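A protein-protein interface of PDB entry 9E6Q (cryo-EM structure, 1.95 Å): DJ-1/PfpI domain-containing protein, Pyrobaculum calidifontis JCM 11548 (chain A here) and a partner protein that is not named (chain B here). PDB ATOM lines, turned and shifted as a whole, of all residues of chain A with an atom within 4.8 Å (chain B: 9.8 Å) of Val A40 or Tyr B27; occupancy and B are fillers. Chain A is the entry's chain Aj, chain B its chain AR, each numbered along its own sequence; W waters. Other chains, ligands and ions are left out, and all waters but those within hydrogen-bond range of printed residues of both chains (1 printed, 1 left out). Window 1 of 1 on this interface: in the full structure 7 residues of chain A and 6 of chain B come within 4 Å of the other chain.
Printed residues of chain A that touch a printed residue of chain B: Arg A38, Asp A39, Val A40, Asn A41 and Val A42.
Along chain A the printed residues that touch a printed residue of chain B span positions 38 to 42.
Hydrophobic or aromatic side chains of chain B within 4 Å of the printed part of chain A: Tyr B27, Leu B30, Ile B50 and Val B53.
Among the printed residues, 9 pairs touch across the chains.
Among the printed residues, no Asp or Glu carboxylate lies within 4 Å of a Lys or Arg side-chain nitrogen of the other chain.
Val A8 touches none of the printed residues of chain B.
No residue of chain B comes within 4 Å of Ser A37.
Of the printed residues of chain B, Arg A38 touches Tyr B27 (3.6 Å), Leu B30 (3.9 Å), Ile B50 (3.7 Å) and Val B53 (3.99 Å).
Of chain B, only Tyr B27 (3.6 Å) comes within 4 Å of Asp A39.
Of chain B, only Tyr B27 comes within 4 Å of Val A40.
Of chain B, only Arg B25 and Tyr B27 come within 4 Å of Asn A41.
Of chain B, only Arg B25 (3.8 Å) comes within 4 Å of Val A42.
Tyr B27 touches just these residues of chain A: Arg A38, Asp A39, Val A40 and Asn A41.
Of the printed residues of chain A, Leu B30 touches Arg A38 (3.9 Å).
Val B33 touches none of the printed residues of chain A.
Of the printed residues of chain A, Ile B50 touches Arg A38 (3.7 Å).
Printed residues of chain A within 4 Å of Val B53: Arg A38.
The backbone carbonyl oxygen (O) of Asn A41 lies within hydrogen-bond range of the guanidinium group (NH2) of Arg B25 (3.3 Å).
The guanidinium group (NH1) of Arg B25 lies within salt-bridge range of the side-chain carboxylate (OD2) of Asp B28 (3.0 Å).
The side-chain carboxylate of Asp A39 lies within hydrogen-bond range of the side-chain hydroxyl of Ser A37 (2.8 Å).
Water W1 lies within hydrogen-bond range of O of Val A42 (2.7 Å), O of Val A40 (2.7 Å) and NE of Arg B25 (2.8 Å).
CD2 of Tyr B27 touches O of Arg A38 (3.6 Å).
CD1 of Leu B30 touches NE of Arg A38, at 3.9 Å.
CG2 of Ile B50 touches NH2 of Arg A38, at 3.7 Å.
Val B53 touches Arg A38 (CG2 to CD, 3.99 Å).
Asp A39 touches Tyr B27 (O to CE2, 3.6 Å).
O of Val A40 touches CB of Tyr B27, 3.5 Å away.
CB of Asn A41 touches CZ of Tyr B27, at 3.3 Å.
Val A42 touches Arg B25 (O to NE, 3.8 Å).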
ATOM      1  N   VAL A   8       9.118  18.170  33.286  1.00  0.00           N
ATOM      2  CA  VAL A   8       8.953  17.685  31.918  1.00  0.00           C
ATOM      3  C   VAL A   8       9.407  18.817  31.006  1.00  0.00           C
ATOM      4  O   VAL A   8       8.640  19.704  30.646  1.00  0.00           O
ATOM      5  CB  VAL A   8       7.520  17.246  31.632  1.00  0.00           C
ATOM      6  CG1 VAL A   8       7.403  16.719  30.219  1.00  0.00           C
ATOM      7  CG2 VAL A   8       7.084  16.199  32.626  1.00  0.00           C
ATOM      8  N   ILE A   9      10.686  18.791  30.642  1.00  0.00           N
ATOM      9  CA  ILE A   9      11.227  19.793  29.734  1.00  0.00           C
ATOM     10  C   ILE A   9      10.761  19.526  28.309  1.00  0.00           C
ATOM     11  O   ILE A   9      10.460  20.455  27.554  1.00  0.00           O
ATOM     12  CB  ILE A   9      12.760  19.816  29.839  1.00  0.00           C
ATOM     13  CG1 ILE A   9      13.186  20.570  31.094  1.00  0.00           C
ATOM     14  CG2 ILE A   9      13.383  20.444  28.614  1.00  0.00           C
ATOM     15  CD1 ILE A   9      14.266  19.875  31.861  1.00  0.00           C
ATOM     16  N   ASP A  10      10.688  18.258  27.923  1.00  0.00           N
ATOM     17  CA  ASP A  10      10.458  17.889  26.538  1.00  0.00           C
ATOM     18  C   ASP A  10       9.672  16.589  26.496  1.00  0.00           C
ATOM     19  O   ASP A  10       9.736  15.774  27.417  1.00  0.00           O
ATOM     20  CB  ASP A  10      11.794  17.761  25.796  1.00  0.00           C
ATOM     21  CG  ASP A  10      11.630  17.401  24.340  1.00  0.00           C
ATOM     22  OD1 ASP A  10      11.155  18.247  23.559  1.00  0.00           O
ATOM     23  OD2 ASP A  10      12.012  16.277  23.969  1.00  0.00           O
ATOM     24  N   THR A  11       8.913  16.408  25.415  1.00  0.00           N
ATOM     25  CA  THR A  11       8.191  15.166  25.181  1.00  0.00           C
ATOM     26  C   THR A  11       8.516  14.519  23.841  1.00  0.00           C
ATOM     27  O   THR A  11       7.796  13.604  23.434  1.00  0.00           O
ATOM     28  CB  THR A  11       6.668  15.384  25.269  1.00  0.00           C
ATOM     29  OG1 THR A  11       6.189  15.967  24.051  1.00  0.00           O
ATOM     30  CG2 THR A  11       6.297  16.280  26.440  1.00  0.00           C
ATOM     31  N   VAL A  35       6.191  22.034  34.456  1.00  0.00           N
ATOM     32  CA  VAL A  35       6.378  22.347  33.044  1.00  0.00           C
ATOM     33  C   VAL A  35       6.914  23.764  32.930  1.00  0.00           C
ATOM     34  O   VAL A  35       6.473  24.662  33.651  1.00  0.00           O
ATOM     35  CB  VAL A  35       5.060  22.181  32.259  1.00  0.00           C
ATOM     36  CG1 VAL A  35       5.146  22.846  30.912  1.00  0.00           C
ATOM     37  CG2 VAL A  35       4.733  20.718  32.092  1.00  0.00           C
ATOM     38  N   SER A  37       7.522  25.252  29.611  1.00  0.00           N
ATOM     39  CA  SER A  37       7.412  25.685  28.229  1.00  0.00           C
ATOM     40  C   SER A  37       5.988  25.464  27.746  1.00  0.00           C
ATOM     41  O   SER A  37       5.260  24.631  28.284  1.00  0.00           O
ATOM     42  CB  SER A  37       8.402  24.938  27.331  1.00  0.00           C
ATOM     43  OG  SER A  37       7.973  23.614  27.098  1.00  0.00           O
ATOM     44  N   ARG A  38       5.598  26.217  26.723  1.00  0.00           N
ATOM     45  CA  ARG A  38       4.235  26.140  26.214  1.00  0.00           C
ATOM     46  C   ARG A  38       4.017  24.987  25.247  1.00  0.00           C
ATOM     47  O   ARG A  38       2.874  24.739  24.857  1.00  0.00           O
ATOM     48  CB  ARG A  38       3.857  27.452  25.529  1.00  0.00           C
ATOM     49  CG  ARG A  38       4.314  28.691  26.268  1.00  0.00           C
ATOM     50  CD  ARG A  38       4.139  29.934  25.419  1.00  0.00           C
ATOM     51  NE  ARG A  38       4.694  29.764  24.083  1.00  0.00           N
ATOM     52  CZ  ARG A  38       5.329  30.712  23.407  1.00  0.00           C
ATOM     53  NH1 ARG A  38       5.515  31.918  23.919  1.00  0.00           N
ATOM     54  NH2 ARG A  38       5.783  30.444  22.186  1.00  0.00           N
ATOM     55  N   ASP A  39       5.068  24.274  24.857  1.00  0.00           N
ATOM     56  CA  ASP A  39       4.935  23.221  23.864  1.00  0.00           C
ATOM     57  C   ASP A  39       4.673  21.847  24.460  1.00  0.00           C
ATOM     58  O   ASP A  39       4.393  20.912  23.707  1.00  0.00           O
ATOM     59  CB  ASP A  39       6.193  23.156  23.003  1.00  0.00           C
ATOM     60  CG  ASP A  39       7.447  23.014  23.828  1.00  0.00           C
ATOM     61  OD1 ASP A  39       7.941  24.036  24.338  1.00  0.00           O
ATOM     62  OD2 ASP A  39       7.942  21.882  23.971  1.00  0.00           O
ATOM     63  N   VAL A  40       4.766  21.694  25.773  1.00  0.00           N
ATOM     64  CA  VAL A  40       4.543  20.402  26.411  1.00  0.00           C
ATOM     65  C   VAL A  40       3.046  20.182  26.579  1.00  0.00           C
ATOM     66  O   VAL A  40       2.323  21.077  27.028  1.00  0.00           O
ATOM     67  CB  VAL A  40       5.279  20.332  27.757  1.00  0.00           C
ATOM     68  CG1 VAL A  40       4.757  19.187  28.584  1.00  0.00           C
ATOM     69  CG2 VAL A  40       6.765  20.178  27.528  1.00  0.00           C
ATOM     70  N   ASN A  41       2.574  18.993  26.213  1.00  0.00           N
ATOM     71  CA  ASN A  41       1.149  18.720  26.122  1.00  0.00           C
ATOM     72  C   ASN A  41       0.572  18.020  27.343  1.00  0.00           C
ATOM     73  O   ASN A  41      -0.623  17.726  27.355  1.00  0.00           O
ATOM     74  CB  ASN A  41       0.862  17.876  24.880  1.00  0.00           C
ATOM     75  CG  ASN A  41       1.275  16.435  25.045  1.00  0.00           C
ATOM     76  OD1 ASN A  41       0.470  15.582  25.408  1.00  0.00           O
ATOM     77  ND2 ASN A  41       2.543  16.157  24.802  1.00  0.00           N
ATOM     78  N   VAL A  42       1.363  17.751  28.355  1.00  0.00           N
ATOM     79  CA  VAL A  42       0.909  16.936  29.474  1.00  0.00           C
ATOM     80  C   VAL A  42       0.360  17.831  30.570  1.00  0.00           C
ATOM     81  O   VAL A  42       0.691  19.014  30.668  1.00  0.00           O
ATOM     82  CB  VAL A  42       2.036  16.025  30.005  1.00  0.00           C
ATOM     83  CG1 VAL A  42       2.760  15.375  28.851  1.00  0.00           C
ATOM     84  CG2 VAL A  42       2.997  16.802  30.877  1.00  0.00           C
ATOM     85  N   TYR B   5      -6.203  33.663  27.328  1.00  0.00           N
ATOM     86  CA  TYR B   5      -4.821  33.892  26.950  1.00  0.00           C
ATOM     87  C   TYR B   5      -4.776  34.880  25.798  1.00  0.00           C
ATOM     88  O   TYR B   5      -5.454  34.691  24.785  1.00  0.00           O
ATOM     89  CB  TYR B   5      -4.137  32.583  26.562  1.00  0.00           C
ATOM     90  CG  TYR B   5      -3.941  31.658  27.731  1.00  0.00           C
ATOM     91  CD1 TYR B   5      -2.812  31.744  28.522  1.00  0.00           C
ATOM     92  CD2 TYR B   5      -4.894  30.712  28.053  1.00  0.00           C
ATOM     93  CE1 TYR B   5      -2.634  30.912  29.591  1.00  0.00           C
ATOM     94  CE2 TYR B   5      -4.725  29.874  29.122  1.00  0.00           C
ATOM     95  CZ  TYR B   5      -3.591  29.978  29.889  1.00  0.00           C
ATOM     96  OH  TYR B   5      -3.416  29.142  30.961  1.00  0.00           O
ATOM     97  N   VAL B   7      -2.732  36.092  22.841  1.00  0.00           N
ATOM     98  CA  VAL B   7      -1.683  35.547  21.993  1.00  0.00           C
ATOM     99  C   VAL B   7      -1.325  36.595  20.952  1.00  0.00           C
ATOM    100  O   VAL B   7      -2.174  37.000  20.152  1.00  0.00           O
ATOM    101  CB  VAL B   7      -2.116  34.234  21.328  1.00  0.00           C
ATOM    102  CG1 VAL B   7      -0.983  33.662  20.516  1.00  0.00           C
ATOM    103  CG2 VAL B   7      -2.573  33.240  22.372  1.00  0.00           C
ATOM    104  N   VAL B  21      -7.849  33.789  23.449  1.00  0.00           N
ATOM    105  CA  VAL B  21      -8.280  32.405  23.350  1.00  0.00           C
ATOM    106  C   VAL B  21      -8.473  31.866  24.755  1.00  0.00           C
ATOM    107  O   VAL B  21      -7.626  32.073  25.627  1.00  0.00           O
ATOM    108  CB  VAL B  21      -7.259  31.559  22.566  1.00  0.00           C
ATOM    109  CG1 VAL B  21      -7.608  30.101  22.646  1.00  0.00           C
ATOM    110  CG2 VAL B  21      -7.207  32.007  21.128  1.00  0.00           C
ATOM    111  N   VAL B  22      -9.588  31.193  24.978  1.00  0.00           N
ATOM    112  CA  VAL B  22      -9.887  30.604  26.274  1.00  0.00           C
ATOM    113  C   VAL B  22      -9.400  29.164  26.278  1.00  0.00           C
ATOM    114  O   VAL B  22      -9.715  28.387  25.371  1.00  0.00           O
ATOM    115  CB  VAL B  22     -11.390  30.679  26.579  1.00  0.00           C
ATOM    116  CG1 VAL B  22     -11.683  30.046  27.914  1.00  0.00           C
ATOM    117  CG2 VAL B  22     -11.844  32.117  26.567  1.00  0.00           C
ATOM    118  N   GLY B  23      -8.617  28.808  27.290  1.00  0.00           N
ATOM    119  CA  GLY B  23      -8.138  27.447  27.400  1.00  0.00           C
ATOM    120  C   GLY B  23      -7.756  27.112  28.821  1.00  0.00           C
ATOM    121  O   GLY B  23      -7.672  27.978  29.692  1.00  0.00           O
ATOM    122  N   GLU B  24      -7.523  25.822  29.042  1.00  0.00           N
ATOM    123  CA  GLU B  24      -7.078  25.355  30.346  1.00  0.00           C
ATOM    124  C   GLU B  24      -5.631  25.740  30.619  1.00  0.00           C
ATOM    125  O   GLU B  24      -5.308  26.218  31.709  1.00  0.00           O
ATOM    126  CB  GLU B  24      -7.253  23.841  30.431  1.00  0.00           C
ATOM    127  CG  GLU B  24      -7.213  23.302  31.831  1.00  0.00           C
ATOM    128  CD  GLU B  24      -8.585  23.200  32.431  1.00  0.00           C
ATOM    129  OE1 GLU B  24      -9.551  23.157  31.650  1.00  0.00           O
ATOM    130  OE2 GLU B  24      -8.704  23.173  33.675  1.00  0.00           O
ATOM    131  N   ARG B  25      -4.753  25.527  29.647  1.00  0.00           N
ATOM    132  CA  ARG B  25      -3.328  25.784  29.791  1.00  0.00           C
ATOM    133  C   ARG B  25      -2.853  26.493  28.538  1.00  0.00           C
ATOM    134  O   ARG B  25      -3.549  26.499  27.517  1.00  0.00           O
ATOM    135  CB  ARG B  25      -2.539  24.487  30.000  1.00  0.00           C
ATOM    136  CG  ARG B  25      -3.257  23.423  30.780  1.00  0.00           C
ATOM    137  CD  ARG B  25      -2.342  22.233  31.034  1.00  0.00           C
ATOM    138  NE  ARG B  25      -2.204  21.330  29.897  1.00  0.00           N
ATOM    139  CZ  ARG B  25      -3.195  20.673  29.312  1.00  0.00           C
ATOM    140  NH1 ARG B  25      -4.441  20.766  29.744  1.00  0.00           N
ATOM    141  NH2 ARG B  25      -2.925  19.881  28.280  1.00  0.00           N
ATOM    142  N   PRO B  26      -1.667  27.103  28.578  1.00  0.00           N
ATOM    143  CA  PRO B  26      -1.142  27.723  27.353  1.00  0.00           C
ATOM    144  C   PRO B  26      -1.021  26.763  26.184  1.00  0.00           C
ATOM    145  O   PRO B  26      -1.141  27.191  25.032  1.00  0.00           O
ATOM    146  CB  PRO B  26       0.222  28.255  27.798  1.00  0.00           C
ATOM    147  CG  PRO B  26       0.063  28.510  29.228  1.00  0.00           C
ATOM    148  CD  PRO B  26      -0.860  27.461  29.754  1.00  0.00           C
ATOM    149  N   TYR B  27      -0.781  25.476  26.436  1.00  0.00           N
ATOM    150  CA  TYR B  27      -0.684  24.528  25.332  1.00  0.00           C
ATOM    151  C   TYR B  27      -2.014  24.379  24.606  1.00  0.00           C
ATOM    152  O   TYR B  27      -2.050  24.336  23.373  1.00  0.00           O
ATOM    153  CB  TYR B  27      -0.193  23.173  25.835  1.00  0.00           C
ATOM    154  CG  TYR B  27      -0.207  22.110  24.769  1.00  0.00           C
ATOM    155  CD1 TYR B  27      -1.299  21.270  24.613  1.00  0.00           C
ATOM    156  CD2 TYR B  27       0.854  21.970  23.893  1.00  0.00           C
ATOM    157  CE1 TYR B  27      -1.323  20.317  23.634  1.00  0.00           C
ATOM    158  CE2 TYR B  27       0.840  21.018  22.915  1.00  0.00           C
ATOM    159  CZ  TYR B  27      -0.252  20.195  22.785  1.00  0.00           C
ATOM    160  OH  TYR B  27      -0.266  19.234  21.805  1.00  0.00           O
ATOM    161  N   ASP B  28      -3.115  24.289  25.353  1.00  0.00           N
ATOM    162  CA  ASP B  28      -4.426  24.157  24.728  1.00  0.00           C
ATOM    163  C   ASP B  28      -4.777  25.397  23.925  1.00  0.00           C
ATOM    164  O   ASP B  28      -5.314  25.297  22.819  1.00  0.00           O
ATOM    165  CB  ASP B  28      -5.495  23.910  25.788  1.00  0.00           C
ATOM    166  CG  ASP B  28      -5.111  22.828  26.750  1.00  0.00           C
ATOM    167  OD1 ASP B  28      -5.148  21.647  26.363  1.00  0.00           O
ATOM    168  OD2 ASP B  28      -4.773  23.158  27.903  1.00  0.00           O
ATOM    169  N   ALA B  29      -4.487  26.575  24.474  1.00  0.00           N
ATOM    170  CA  ALA B  29      -4.780  27.815  23.770  1.00  0.00           C
ATOM    171  C   ALA B  29      -3.980  27.919  22.481  1.00  0.00           C
ATOM    172  O   ALA B  29      -4.480  28.421  21.472  1.00  0.00           O
ATOM    173  CB  ALA B  29      -4.499  29.011  24.675  1.00  0.00           C
ATOM    174  N   LEU B  30      -2.729  27.466  22.501  1.00  0.00           N
ATOM    175  CA  LEU B  30      -1.915  27.519  21.292  1.00  0.00           C
ATOM    176  C   LEU B  30      -2.416  26.539  20.240  1.00  0.00           C
ATOM    177  O   LEU B  30      -2.344  26.823  19.041  1.00  0.00           O
ATOM    178  CB  LEU B  30      -0.455  27.248  21.633  1.00  0.00           C
ATOM    179  CG  LEU B  30       0.311  28.423  22.237  1.00  0.00           C
ATOM    180  CD1 LEU B  30       1.789  28.243  22.010  1.00  0.00           C
ATOM    181  CD2 LEU B  30      -0.156  29.732  21.649  1.00  0.00           C
ATOM    182  N   GLU B  31      -2.932  25.385  20.661  1.00  0.00           N
ATOM    183  CA  GLU B  31      -3.483  24.440  19.697  1.00  0.00           C
ATOM    184  C   GLU B  31      -4.668  25.043  18.961  1.00  0.00           C
ATOM    185  O   GLU B  31      -4.819  24.854  17.751  1.00  0.00           O
ATOM    186  CB  GLU B  31      -3.895  23.146  20.391  1.00  0.00           C
ATOM    187  CG  GLU B  31      -2.741  22.326  20.916  1.00  0.00           C
ATOM    188  CD  GLU B  31      -1.723  22.001  19.848  1.00  0.00           C
ATOM    189  OE1 GLU B  31      -2.002  21.117  19.013  1.00  0.00           O
ATOM    190  OE2 GLU B  31      -0.643  22.627  19.842  1.00  0.00           O
ATOM    191  N   LYS B  32      -5.520  25.770  19.679  1.00  0.00           N
ATOM    192  CA  LYS B  32      -6.635  26.445  19.032  1.00  0.00           C
ATOM    193  C   LYS B  32      -6.145  27.502  18.053  1.00  0.00           C
ATOM    194  O   LYS B  32      -6.710  27.658  16.968  1.00  0.00           O
ATOM    195  CB  LYS B  32      -7.556  27.061  20.082  1.00  0.00           C
ATOM    196  CG  LYS B  32      -9.025  26.812  19.822  1.00  0.00           C
ATOM    197  CD  LYS B  32      -9.902  27.777  20.594  1.00  0.00           C
ATOM    198  CE  LYS B  32      -9.902  27.475  22.077  1.00  0.00           C
ATOM    199  NZ  LYS B  32     -11.267  27.576  22.653  1.00  0.00           N
ATOM    200  N   VAL B  33      -5.095  28.236  18.415  1.00  0.00           N
ATOM    201  CA  VAL B  33      -4.573  29.269  17.525  1.00  0.00           C
ATOM    202  C   VAL B  33      -4.017  28.653  16.250  1.00  0.00           C
ATOM    203  O   VAL B  33      -4.240  29.166  15.150  1.00  0.00           O
ATOM    204  CB  VAL B  33      -3.513  30.114  18.252  1.00  0.00           C
ATOM    205  CG1 VAL B  33      -2.841  31.055  17.282  1.00  0.00           C
ATOM    206  CG2 VAL B  33      -4.149  30.885  19.374  1.00  0.00           C
ATOM    207  N   TYR B  34      -3.278  27.552  16.373  1.00  0.00           N
ATOM    208  CA  TYR B  34      -2.679  26.932  15.198  1.00  0.00           C
ATOM    209  C   TYR B  34      -3.741  26.374  14.263  1.00  0.00           C
ATOM    210  O   TYR B  34      -3.655  26.542  13.044  1.00  0.00           O
ATOM    211  CB  TYR B  34      -1.728  25.822  15.620  1.00  0.00           C
ATOM    212  CG  TYR B  34      -0.383  26.310  16.067  1.00  0.00           C
ATOM    213  CD1 TYR B  34       0.360  27.172  15.286  1.00  0.00           C
ATOM    214  CD2 TYR B  34       0.154  25.890  17.267  1.00  0.00           C
ATOM    215  CE1 TYR B  34       1.597  27.612  15.697  1.00  0.00           C
ATOM    216  CE2 TYR B  34       1.380  26.323  17.684  1.00  0.00           C
ATOM    217  CZ  TYR B  34       2.100  27.182  16.898  1.00  0.00           C
ATOM    218  OH  TYR B  34       3.331  27.609  17.323  1.00  0.00           O
ATOM    219  N   SER B  35      -4.746  25.702  14.813  1.00  0.00           N
ATOM    220  CA  SER B  35      -5.753  25.069  13.978  1.00  0.00           C
ATOM    221  C   SER B  35      -6.708  26.076  13.359  1.00  0.00           C
ATOM    222  O   SER B  35      -7.129  25.898  12.216  1.00  0.00           O
ATOM    223  CB  SER B  35      -6.525  24.035  14.791  1.00  0.00           C
ATOM    224  OG  SER B  35      -7.524  24.650  15.577  1.00  0.00           O
ATOM    225  N   ARG B  45       1.847  25.600  10.194  1.00  0.00           N
ATOM    226  CA  ARG B  45       2.306  25.930  11.536  1.00  0.00           C
ATOM    227  C   ARG B  45       3.675  26.593  11.504  1.00  0.00           C
ATOM    228  O   ARG B  45       3.965  27.471  12.322  1.00  0.00           O
ATOM    229  CB  ARG B  45       2.321  24.678  12.404  1.00  0.00           C
ATOM    230  CG  ARG B  45       1.071  24.510  13.232  1.00  0.00           C
ATOM    231  CD  ARG B  45       0.752  23.064  13.523  1.00  0.00           C
ATOM    232  NE  ARG B  45      -0.686  22.838  13.563  1.00  0.00           N
ATOM    233  CZ  ARG B  45      -1.368  22.498  14.647  1.00  0.00           C
ATOM    234  NH1 ARG B  45      -0.769  22.316  15.809  1.00  0.00           N
ATOM    235  NH2 ARG B  45      -2.683  22.337  14.562  1.00  0.00           N
ATOM    236  N   ILE B  50       4.582  32.644  17.073  1.00  0.00           N
ATOM    237  CA  ILE B  50       3.982  33.115  18.315  1.00  0.00           C
ATOM    238  C   ILE B  50       5.009  33.955  19.062  1.00  0.00           C
ATOM    239  O   ILE B  50       6.109  33.486  19.359  1.00  0.00           O
ATOM    240  CB  ILE B  50       3.498  31.938  19.172  1.00  0.00           C
ATOM    241  CG1 ILE B  50       2.351  31.210  18.473  1.00  0.00           C
ATOM    242  CG2 ILE B  50       3.066  32.415  20.531  1.00  0.00           C
ATOM    243  CD1 ILE B  50       1.276  32.111  17.961  1.00  0.00           C
ATOM    244  N   VAL B  53       2.508  35.128  24.871  1.00  0.00           N
ATOM    245  CA  VAL B  53       1.306  34.521  25.427  1.00  0.00           C
ATOM    246  C   VAL B  53       1.187  34.980  26.870  1.00  0.00           C
ATOM    247  O   VAL B  53       2.134  34.837  27.649  1.00  0.00           O
ATOM    248  CB  VAL B  53       1.348  32.984  25.348  1.00  0.00           C
ATOM    249  CG1 VAL B  53       0.099  32.386  25.946  1.00  0.00           C
ATOM    250  CG2 VAL B  53       1.511  32.530  23.917  1.00  0.00           C
HETATM  251  O   HOH W   1       0.458  21.095  28.992  1.00  0.00           O
